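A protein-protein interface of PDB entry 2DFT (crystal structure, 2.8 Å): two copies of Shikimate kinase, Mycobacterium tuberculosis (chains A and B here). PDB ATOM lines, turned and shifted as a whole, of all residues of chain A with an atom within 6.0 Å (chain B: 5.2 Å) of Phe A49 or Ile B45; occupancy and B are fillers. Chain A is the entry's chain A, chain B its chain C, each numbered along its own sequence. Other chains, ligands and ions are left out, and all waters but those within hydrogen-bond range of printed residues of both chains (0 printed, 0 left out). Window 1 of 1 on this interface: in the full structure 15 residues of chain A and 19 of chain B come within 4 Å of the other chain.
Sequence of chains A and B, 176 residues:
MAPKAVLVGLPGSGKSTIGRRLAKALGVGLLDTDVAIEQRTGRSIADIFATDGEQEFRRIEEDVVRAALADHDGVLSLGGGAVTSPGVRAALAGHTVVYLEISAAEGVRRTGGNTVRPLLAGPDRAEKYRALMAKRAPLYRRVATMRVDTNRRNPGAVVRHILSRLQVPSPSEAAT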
ATOM      1  N   SER A  44      -8.512  27.011   0.360  1.00  0.00           N
ATOM      2  CA  SER A  44      -8.354  25.668  -0.208  1.00  0.00           C
ATOM      3  C   SER A  44      -6.952  25.221   0.068  1.00  0.00           C
ATOM      4  O   SER A  44      -6.049  26.069   0.055  1.00  0.00           O
ATOM      5  CB  SER A  44      -8.444  25.720  -1.730  1.00  0.00           C
ATOM      6  OG  SER A  44      -7.159  25.633  -2.333  1.00  0.00           O
ATOM      7  N   ILE A  45      -6.814  23.912   0.330  1.00  0.00           N
ATOM      8  CA  ILE A  45      -5.558  23.267   0.703  1.00  0.00           C
ATOM      9  C   ILE A  45      -4.464  23.568  -0.326  1.00  0.00           C
ATOM     10  O   ILE A  45      -3.321  23.899   0.091  1.00  0.00           O
ATOM     11  CB  ILE A  45      -5.706  21.784   0.941  1.00  0.00           C
ATOM     12  CG1 ILE A  45      -5.875  21.625   2.432  1.00  0.00           C
ATOM     13  CG2 ILE A  45      -4.495  21.071   0.449  1.00  0.00           C
ATOM     14  CD1 ILE A  45      -6.279  20.256   2.964  1.00  0.00           C
ATOM     15  N   ALA A  46      -4.880  23.600  -1.613  1.00  0.00           N
ATOM     16  CA  ALA A  46      -4.005  24.113  -2.689  1.00  0.00           C
ATOM     17  C   ALA A  46      -3.662  25.575  -2.470  1.00  0.00           C
ATOM     18  O   ALA A  46      -2.488  25.875  -2.200  1.00  0.00           O
ATOM     19  CB  ALA A  46      -4.478  23.878  -4.075  1.00  0.00           C
ATOM     20  N   ASP A  47      -4.631  26.473  -2.309  1.00  0.00           N
ATOM     21  CA  ASP A  47      -4.221  27.779  -1.718  1.00  0.00           C
ATOM     22  C   ASP A  47      -3.142  27.885  -0.626  1.00  0.00           C
ATOM     23  O   ASP A  47      -2.703  28.997  -0.251  1.00  0.00           O
ATOM     24  CB  ASP A  47      -5.385  28.719  -1.440  1.00  0.00           C
ATOM     25  CG  ASP A  47      -6.277  28.836  -2.635  1.00  0.00           C
ATOM     26  OD1 ASP A  47      -5.864  28.241  -3.659  1.00  0.00           O
ATOM     27  OD2 ASP A  47      -7.322  29.521  -2.565  1.00  0.00           O
ATOM     28  N   ILE A  48      -2.770  26.772  -0.016  1.00  0.00           N
ATOM     29  CA  ILE A  48      -2.022  26.970   1.213  1.00  0.00           C
ATOM     30  C   ILE A  48      -0.683  26.468   0.830  1.00  0.00           C
ATOM     31  O   ILE A  48       0.251  27.228   0.893  1.00  0.00           O
ATOM     32  CB  ILE A  48      -2.662  26.254   2.449  1.00  0.00           C
ATOM     33  CG1 ILE A  48      -4.042  26.809   2.763  1.00  0.00           C
ATOM     34  CG2 ILE A  48      -1.836  26.298   3.731  1.00  0.00           C
ATOM     35  CD1 ILE A  48      -4.809  25.681   3.568  1.00  0.00           C
ATOM     36  N   PHE A  49      -0.626  25.210   0.394  1.00  0.00           N
ATOM     37  CA  PHE A  49       0.565  24.700  -0.269  1.00  0.00           C
ATOM     38  C   PHE A  49       1.014  25.625  -1.395  1.00  0.00           C
ATOM     39  O   PHE A  49       2.031  26.336  -1.177  1.00  0.00           O
ATOM     40  CB  PHE A  49       0.369  23.338  -0.858  1.00  0.00           C
ATOM     41  CG  PHE A  49       0.588  22.235   0.110  1.00  0.00           C
ATOM     42  CD1 PHE A  49       1.858  21.763   0.330  1.00  0.00           C
ATOM     43  CD2 PHE A  49      -0.504  21.563   0.651  1.00  0.00           C
ATOM     44  CE1 PHE A  49       2.069  20.701   1.206  1.00  0.00           C
ATOM     45  CE2 PHE A  49      -0.329  20.566   1.576  1.00  0.00           C
ATOM     46  CZ  PHE A  49       0.982  20.092   1.825  1.00  0.00           C
ATOM     47  N   ALA A  50       0.378  25.615  -2.583  1.00  0.00           N
ATOM     48  CA  ALA A  50       0.773  26.666  -3.592  1.00  0.00           C
ATOM     49  C   ALA A  50       0.976  28.133  -3.146  1.00  0.00           C
ATOM     50  O   ALA A  50       1.442  28.924  -3.965  1.00  0.00           O
ATOM     51  CB  ALA A  50      -0.015  26.655  -4.927  1.00  0.00           C
ATOM     52  N   THR A  51       0.731  28.452  -1.871  1.00  0.00           N
ATOM     53  CA  THR A  51       0.975  29.800  -1.328  1.00  0.00           C
ATOM     54  C   THR A  51       1.895  30.106  -0.129  1.00  0.00           C
ATOM     55  O   THR A  51       2.383  31.234  -0.107  1.00  0.00           O
ATOM     56  CB  THR A  51      -0.368  30.531  -1.186  1.00  0.00           C
ATOM     57  OG1 THR A  51      -0.676  31.120  -2.464  1.00  0.00           O
ATOM     58  CG2 THR A  51      -0.364  31.548  -0.039  1.00  0.00           C
ATOM     59  N   ASP A  52       2.126  29.158   0.804  1.00  0.00           N
ATOM     60  CA  ASP A  52       3.013  29.279   1.992  1.00  0.00           C
ATOM     61  C   ASP A  52       3.767  27.997   2.324  1.00  0.00           C
ATOM     62  O   ASP A  52       4.629  27.991   3.214  1.00  0.00           O
ATOM     63  CB  ASP A  52       2.351  29.850   3.289  1.00  0.00           C
ATOM     64  CG  ASP A  52       0.793  29.987   3.198  1.00  0.00           C
ATOM     65  OD1 ASP A  52       0.071  29.545   4.148  1.00  0.00           O
ATOM     66  OD2 ASP A  52       0.279  30.558   2.185  1.00  0.00           O
ATOM     67  N   GLY A  53       3.454  26.903   1.641  1.00  0.00           N
ATOM     68  CA  GLY A  53       4.395  25.744   1.561  1.00  0.00           C
ATOM     69  C   GLY A  53       4.062  24.556   2.480  1.00  0.00           C
ATOM     70  O   GLY A  53       3.435  24.829   3.514  1.00  0.00           O
ATOM     71  N   GLU A  54       4.474  23.302   2.172  1.00  0.00           N
ATOM     72  CA  GLU A  54       4.648  22.181   3.154  1.00  0.00           C
ATOM     73  C   GLU A  54       4.640  22.600   4.629  1.00  0.00           C
ATOM     74  O   GLU A  54       3.592  22.470   5.271  1.00  0.00           O
ATOM     75  CB  GLU A  54       5.886  21.332   2.873  1.00  0.00           C
ATOM     76  CG  GLU A  54       5.627  20.182   1.988  1.00  0.00           C
ATOM     77  CD  GLU A  54       5.712  18.786   2.713  1.00  0.00           C
ATOM     78  OE1 GLU A  54       6.850  18.265   2.627  1.00  0.00           O
ATOM     79  OE2 GLU A  54       4.729  18.112   3.206  1.00  0.00           O
ATOM     80  N   GLN A  55       5.746  23.207   5.100  1.00  0.00           N
ATOM     81  CA  GLN A  55       6.038  23.694   6.503  1.00  0.00           C
ATOM     82  C   GLN A  55       4.944  24.535   7.193  1.00  0.00           C
ATOM     83  O   GLN A  55       4.443  24.159   8.251  1.00  0.00           O
ATOM     84  CB  GLN A  55       7.457  24.331   6.694  1.00  0.00           C
ATOM     85  CG  GLN A  55       8.462  24.376   5.428  1.00  0.00           C
ATOM     86  CD  GLN A  55       7.760  24.681   4.017  1.00  0.00           C
ATOM     87  OE1 GLN A  55       7.674  23.782   3.128  1.00  0.00           O
ATOM     88  NE2 GLN A  55       7.239  25.945   3.848  1.00  0.00           N
ATOM     89  N   PHE A  57       1.798  24.814   5.901  1.00  0.00           N
ATOM     90  CA  PHE A  57       0.586  24.034   5.841  1.00  0.00           C
ATOM     91  C   PHE A  57       0.608  23.009   6.969  1.00  0.00           C
ATOM     92  O   PHE A  57      -0.387  22.891   7.712  1.00  0.00           O
ATOM     93  CB  PHE A  57       0.399  23.368   4.492  1.00  0.00           C
ATOM     94  CG  PHE A  57      -0.598  22.193   4.500  1.00  0.00           C
ATOM     95  CD1 PHE A  57      -1.933  22.386   4.148  1.00  0.00           C
ATOM     96  CD2 PHE A  57      -0.185  20.896   4.863  1.00  0.00           C
ATOM     97  CE1 PHE A  57      -2.808  21.320   4.086  1.00  0.00           C
ATOM     98  CE2 PHE A  57      -1.019  19.825   4.823  1.00  0.00           C
ATOM     99  CZ  PHE A  57      -2.357  20.041   4.492  1.00  0.00           C
ATOM    100  N   ARG A  58       1.686  22.214   7.055  1.00  0.00           N
ATOM    101  CA  ARG A  58       1.704  21.206   8.110  1.00  0.00           C
ATOM    102  C   ARG A  58       1.539  21.838   9.468  1.00  0.00           C
ATOM    103  O   ARG A  58       1.238  21.152  10.447  1.00  0.00           O
ATOM    104  CB  ARG A  58       2.955  20.341   8.160  1.00  0.00           C
ATOM    105  CG  ARG A  58       3.213  19.383   7.033  1.00  0.00           C
ATOM    106  CD  ARG A  58       1.943  18.778   6.540  1.00  0.00           C
ATOM    107  NE  ARG A  58       2.202  17.958   5.359  1.00  0.00           N
ATOM    108  CZ  ARG A  58       1.325  17.080   4.857  1.00  0.00           C
ATOM    109  NH1 ARG A  58       0.219  16.710   5.546  1.00  0.00           N
ATOM    110  NH2 ARG A  58       1.607  16.525   3.670  1.00  0.00           N
ATOM    111  N   ASP B  34      -4.382  24.788 -10.471  1.00  0.00           N
ATOM    112  CA  ASP B  34      -4.206  23.926  -9.340  1.00  0.00           C
ATOM    113  C   ASP B  34      -5.187  22.769  -9.539  1.00  0.00           C
ATOM    114  O   ASP B  34      -4.709  21.661  -9.686  1.00  0.00           O
ATOM    115  CB  ASP B  34      -4.530  24.685  -8.060  1.00  0.00           C
ATOM    116  CG  ASP B  34      -3.484  25.716  -7.682  1.00  0.00           C
ATOM    117  OD1 ASP B  34      -2.368  25.804  -8.330  1.00  0.00           O
ATOM    118  OD2 ASP B  34      -3.872  26.442  -6.711  1.00  0.00           O
ATOM    119  N   ILE B  37      -3.892  20.225 -11.951  1.00  0.00           N
ATOM    120  CA  ILE B  37      -2.782  19.367 -11.579  1.00  0.00           C
ATOM    121  C   ILE B  37      -3.249  18.039 -11.032  1.00  0.00           C
ATOM    122  O   ILE B  37      -2.897  16.980 -11.561  1.00  0.00           O
ATOM    123  CB  ILE B  37      -1.864  20.131 -10.655  1.00  0.00           C
ATOM    124  CG1 ILE B  37      -1.377  21.299 -11.476  1.00  0.00           C
ATOM    125  CG2 ILE B  37      -0.607  19.328 -10.229  1.00  0.00           C
ATOM    126  CD1 ILE B  37      -0.580  22.276 -10.733  1.00  0.00           C
ATOM    127  N   GLU B  38      -4.057  18.086  -9.974  1.00  0.00           N
ATOM    128  CA  GLU B  38      -4.616  16.844  -9.518  1.00  0.00           C
ATOM    129  C   GLU B  38      -5.627  16.287 -10.526  1.00  0.00           C
ATOM    130  O   GLU B  38      -5.806  15.079 -10.541  1.00  0.00           O
ATOM    131  CB  GLU B  38      -5.175  16.959  -8.124  1.00  0.00           C
ATOM    132  CG  GLU B  38      -5.364  18.380  -7.773  1.00  0.00           C
ATOM    133  CD  GLU B  38      -5.926  18.545  -6.331  1.00  0.00           C
ATOM    134  OE1 GLU B  38      -7.165  18.326  -6.206  1.00  0.00           O
ATOM    135  OE2 GLU B  38      -5.177  18.805  -5.334  1.00  0.00           O
ATOM    136  N   ARG B  43      -3.150  12.911  -8.381  1.00  0.00           N
ATOM    137  CA  ARG B  43      -2.674  12.926  -6.986  1.00  0.00           C
ATOM    138  C   ARG B  43      -2.644  14.297  -6.277  1.00  0.00           C
ATOM    139  O   ARG B  43      -2.288  15.323  -6.813  1.00  0.00           O
ATOM    140  CB  ARG B  43      -1.287  12.321  -6.975  1.00  0.00           C
ATOM    141  CG  ARG B  43      -0.503  12.824  -8.169  1.00  0.00           C
ATOM    142  CD  ARG B  43       0.999  12.274  -8.217  1.00  0.00           C
ATOM    143  NE  ARG B  43       1.517  11.936  -6.904  1.00  0.00           N
ATOM    144  CZ  ARG B  43       2.764  12.139  -6.428  1.00  0.00           C
ATOM    145  NH1 ARG B  43       3.697  12.916  -7.091  1.00  0.00           N
ATOM    146  NH2 ARG B  43       2.990  11.589  -5.170  1.00  0.00           N
ATOM    147  N   SER B  44      -3.020  14.406  -5.035  1.00  0.00           N
ATOM    148  CA  SER B  44      -3.299  15.734  -4.612  1.00  0.00           C
ATOM    149  C   SER B  44      -2.047  16.608  -4.465  1.00  0.00           C
ATOM    150  O   SER B  44      -1.012  16.087  -3.963  1.00  0.00           O
ATOM    151  CB  SER B  44      -4.096  15.646  -3.305  1.00  0.00           C
ATOM    152  OG  SER B  44      -4.661  16.966  -3.067  1.00  0.00           O
ATOM    153  N   ILE B  45      -2.204  17.918  -4.777  1.00  0.00           N
ATOM    154  CA  ILE B  45      -1.188  18.956  -4.578  1.00  0.00           C
ATOM    155  C   ILE B  45      -0.290  18.630  -3.359  1.00  0.00           C
ATOM    156  O   ILE B  45       0.968  18.628  -3.421  1.00  0.00           O
ATOM    157  CB  ILE B  45      -1.728  20.458  -4.696  1.00  0.00           C
ATOM    158  CG1 ILE B  45      -1.508  21.149  -6.046  1.00  0.00           C
ATOM    159  CG2 ILE B  45      -1.076  21.412  -3.702  1.00  0.00           C
ATOM    160  CD1 ILE B  45      -2.511  20.772  -7.046  1.00  0.00           C
ATOM    161  N   ALA B  46      -0.883  18.225  -2.245  1.00  0.00           N
ATOM    162  CA  ALA B  46      -0.026  17.943  -1.079  1.00  0.00           C
ATOM    163  C   ALA B  46       0.848  16.712  -1.333  1.00  0.00           C
ATOM    164  O   ALA B  46       1.971  16.606  -0.841  1.00  0.00           O
ATOM    165  CB  ALA B  46      -0.902  17.671   0.163  1.00  0.00           C
ATOM    166  N   ASP B  47       0.227  15.694  -1.900  1.00  0.00           N
ATOM    167  CA  ASP B  47       0.950  14.446  -2.050  1.00  0.00           C
ATOM    168  C   ASP B  47       1.766  14.750  -3.331  1.00  0.00           C
ATOM    169  O   ASP B  47       1.280  14.484  -4.418  1.00  0.00           O
ATOM    170  CB  ASP B  47      -0.032  13.234  -2.246  1.00  0.00           C
ATOM    171  CG  ASP B  47      -0.727  12.843  -0.942  1.00  0.00           C
ATOM    172  OD1 ASP B  47      -1.959  12.609  -0.880  1.00  0.00           O
ATOM    173  OD2 ASP B  47      -0.020  12.975   0.079  1.00  0.00           O
ATOM    174  N   ILE B  48       2.884  15.478  -3.290  1.00  0.00           N
ATOM    175  CA  ILE B  48       3.547  15.930  -4.539  1.00  0.00           C
ATOM    176  C   ILE B  48       4.605  16.745  -3.872  1.00  0.00           C
ATOM    177  O   ILE B  48       5.802  16.690  -4.250  1.00  0.00           O
ATOM    178  CB  ILE B  48       2.748  16.797  -5.634  1.00  0.00           C
ATOM    179  CG1 ILE B  48       1.759  15.979  -6.534  1.00  0.00           C
ATOM    180  CG2 ILE B  48       3.766  17.473  -6.642  1.00  0.00           C
ATOM    181  CD1 ILE B  48       1.098  16.680  -7.832  1.00  0.00           C
ATOM    182  N   PHE B  49       4.113  17.560  -2.957  1.00  0.00           N
ATOM    183  CA  PHE B  49       4.975  18.374  -2.252  1.00  0.00           C
ATOM    184  C   PHE B  49       5.521  17.398  -1.270  1.00  0.00           C
ATOM    185  O   PHE B  49       6.719  17.356  -1.004  1.00  0.00           O
ATOM    186  CB  PHE B  49       4.152  19.336  -1.471  1.00  0.00           C
ATOM    187  CG  PHE B  49       4.043  20.675  -2.095  1.00  0.00           C
ATOM    188  CD1 PHE B  49       4.895  21.712  -1.670  1.00  0.00           C
ATOM    189  CD2 PHE B  49       3.085  20.905  -3.088  1.00  0.00           C
ATOM    190  CE1 PHE B  49       4.782  23.004  -2.210  1.00  0.00           C
ATOM    191  CE2 PHE B  49       2.967  22.179  -3.631  1.00  0.00           C
ATOM    192  CZ  PHE B  49       3.798  23.233  -3.160  1.00  0.00           C
ATOM    193  N   ALA B  50       4.653  16.692  -0.583  1.00  0.00           N
ATOM    194  CA  ALA B  50       5.238  15.915   0.503  1.00  0.00           C
ATOM    195  C   ALA B  50       5.939  14.730  -0.104  1.00  0.00           C
ATOM    196  O   ALA B  50       6.970  14.280   0.381  1.00  0.00           O
ATOM    197  CB  ALA B  50       4.188  15.487   1.506  1.00  0.00           C
ATOM    198  N   PHE B  57       7.272  20.400  -8.011  1.00  0.00           N
ATOM    199  CA  PHE B  57       5.825  20.566  -8.235  1.00  0.00           C
ATOM    200  C   PHE B  57       5.658  21.696  -9.233  1.00  0.00           C
ATOM    201  O   PHE B  57       4.806  21.679 -10.173  1.00  0.00           O
ATOM    202  CB  PHE B  57       5.085  20.802  -6.905  1.00  0.00           C
ATOM    203  CG  PHE B  57       4.009  21.852  -6.927  1.00  0.00           C
ATOM    204  CD1 PHE B  57       2.690  21.495  -7.202  1.00  0.00           C
ATOM    205  CD2 PHE B  57       4.304  23.172  -6.577  1.00  0.00           C
ATOM    206  CE1 PHE B  57       1.714  22.403  -7.305  1.00  0.00           C
ATOM    207  CE2 PHE B  57       3.284  24.094  -6.613  1.00  0.00           C
ATOM    208  CZ  PHE B  57       1.965  23.687  -6.952  1.00  0.00           C
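The side-chain hydroxyl (OG) of Ser A44 lies close to the backbone NH (N) of Ala A46 (3.1 Å).
The guanidinium group (NE) of Arg A58 is in salt-bridge range of the side-chain carboxylate (OE2) of Glu A54 (3.3 Å).
The backbone NH (N) of Ile B45 lies within hydrogen-bond range of the side-chain carboxylate (OE2) of Glu B38 (3.2 Å).
Among the printed residues, merely in contact across the chains: Ala A46 with Asp B34 (3.7 Å), Phe A49 with Ile B45 (3.7 Å), Phe A49 with Ala B46 (3.3 Å), Phe A49 with Phe B49 (3.4 Å), Glu A54 with Phe B49 (3.7 Å), Glu A54 with Ala B50 (3.2 Å) and Arg A58 with Ala B50 (3.5 Å).
Of chain B, only Ile B45, Ala B46 and Phe B49 come within 4 Å of Phe A49.
Ala A50 touches none of the printed residues of chain B.
Of the printed residues of chain A, Asp B34 touches Ala A46 (3.7 Å).
Ser B44 touches none of the printed residues of chain A.
Of chain A, only Phe A49 (3.7 Å) comes within 4 Å of Ile B45.
Printed residues of chain A within 4 Å of Ala B46: Phe A49.
Of the printed residues of chain A, Phe B49 touches Phe A49 and Glu A54.
The nearest residue of chain A that does not touch Ile B45 is Ala A46 (4.1 Å).
Hydrophobic or aromatic side chains of chain A within 4 Å of the printed part of chain B: Ala A46 and Phe A49.
Of the 12 printed residues of chain B, 5 touch a printed residue of chain A.
Hydrophobic or aromatic side chains of chain B within 4 Å of the printed part of chain A: Ile B45, Ala B46, Phe B49 and Ala B50.
Among the printed residues, no Asp or Glu carboxylate lies within 4 Å of a Lys or Arg side-chain nitrogen of the other chain.
Phe A49 touches Ile B45, but with the chains exchanged Ile A45 does not touch Phe B49 (7.5 Å).
Phe A49 touches Ala B46, but with the chains exchanged Ala A46 does not touch Phe B49 (6.7 Å).
Phe B49 touches its own counterpart, Phe A49.
Of the 7 pairs that touch across the chains among the printed residues, 1 has its exchanged pair printed and touching as well.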
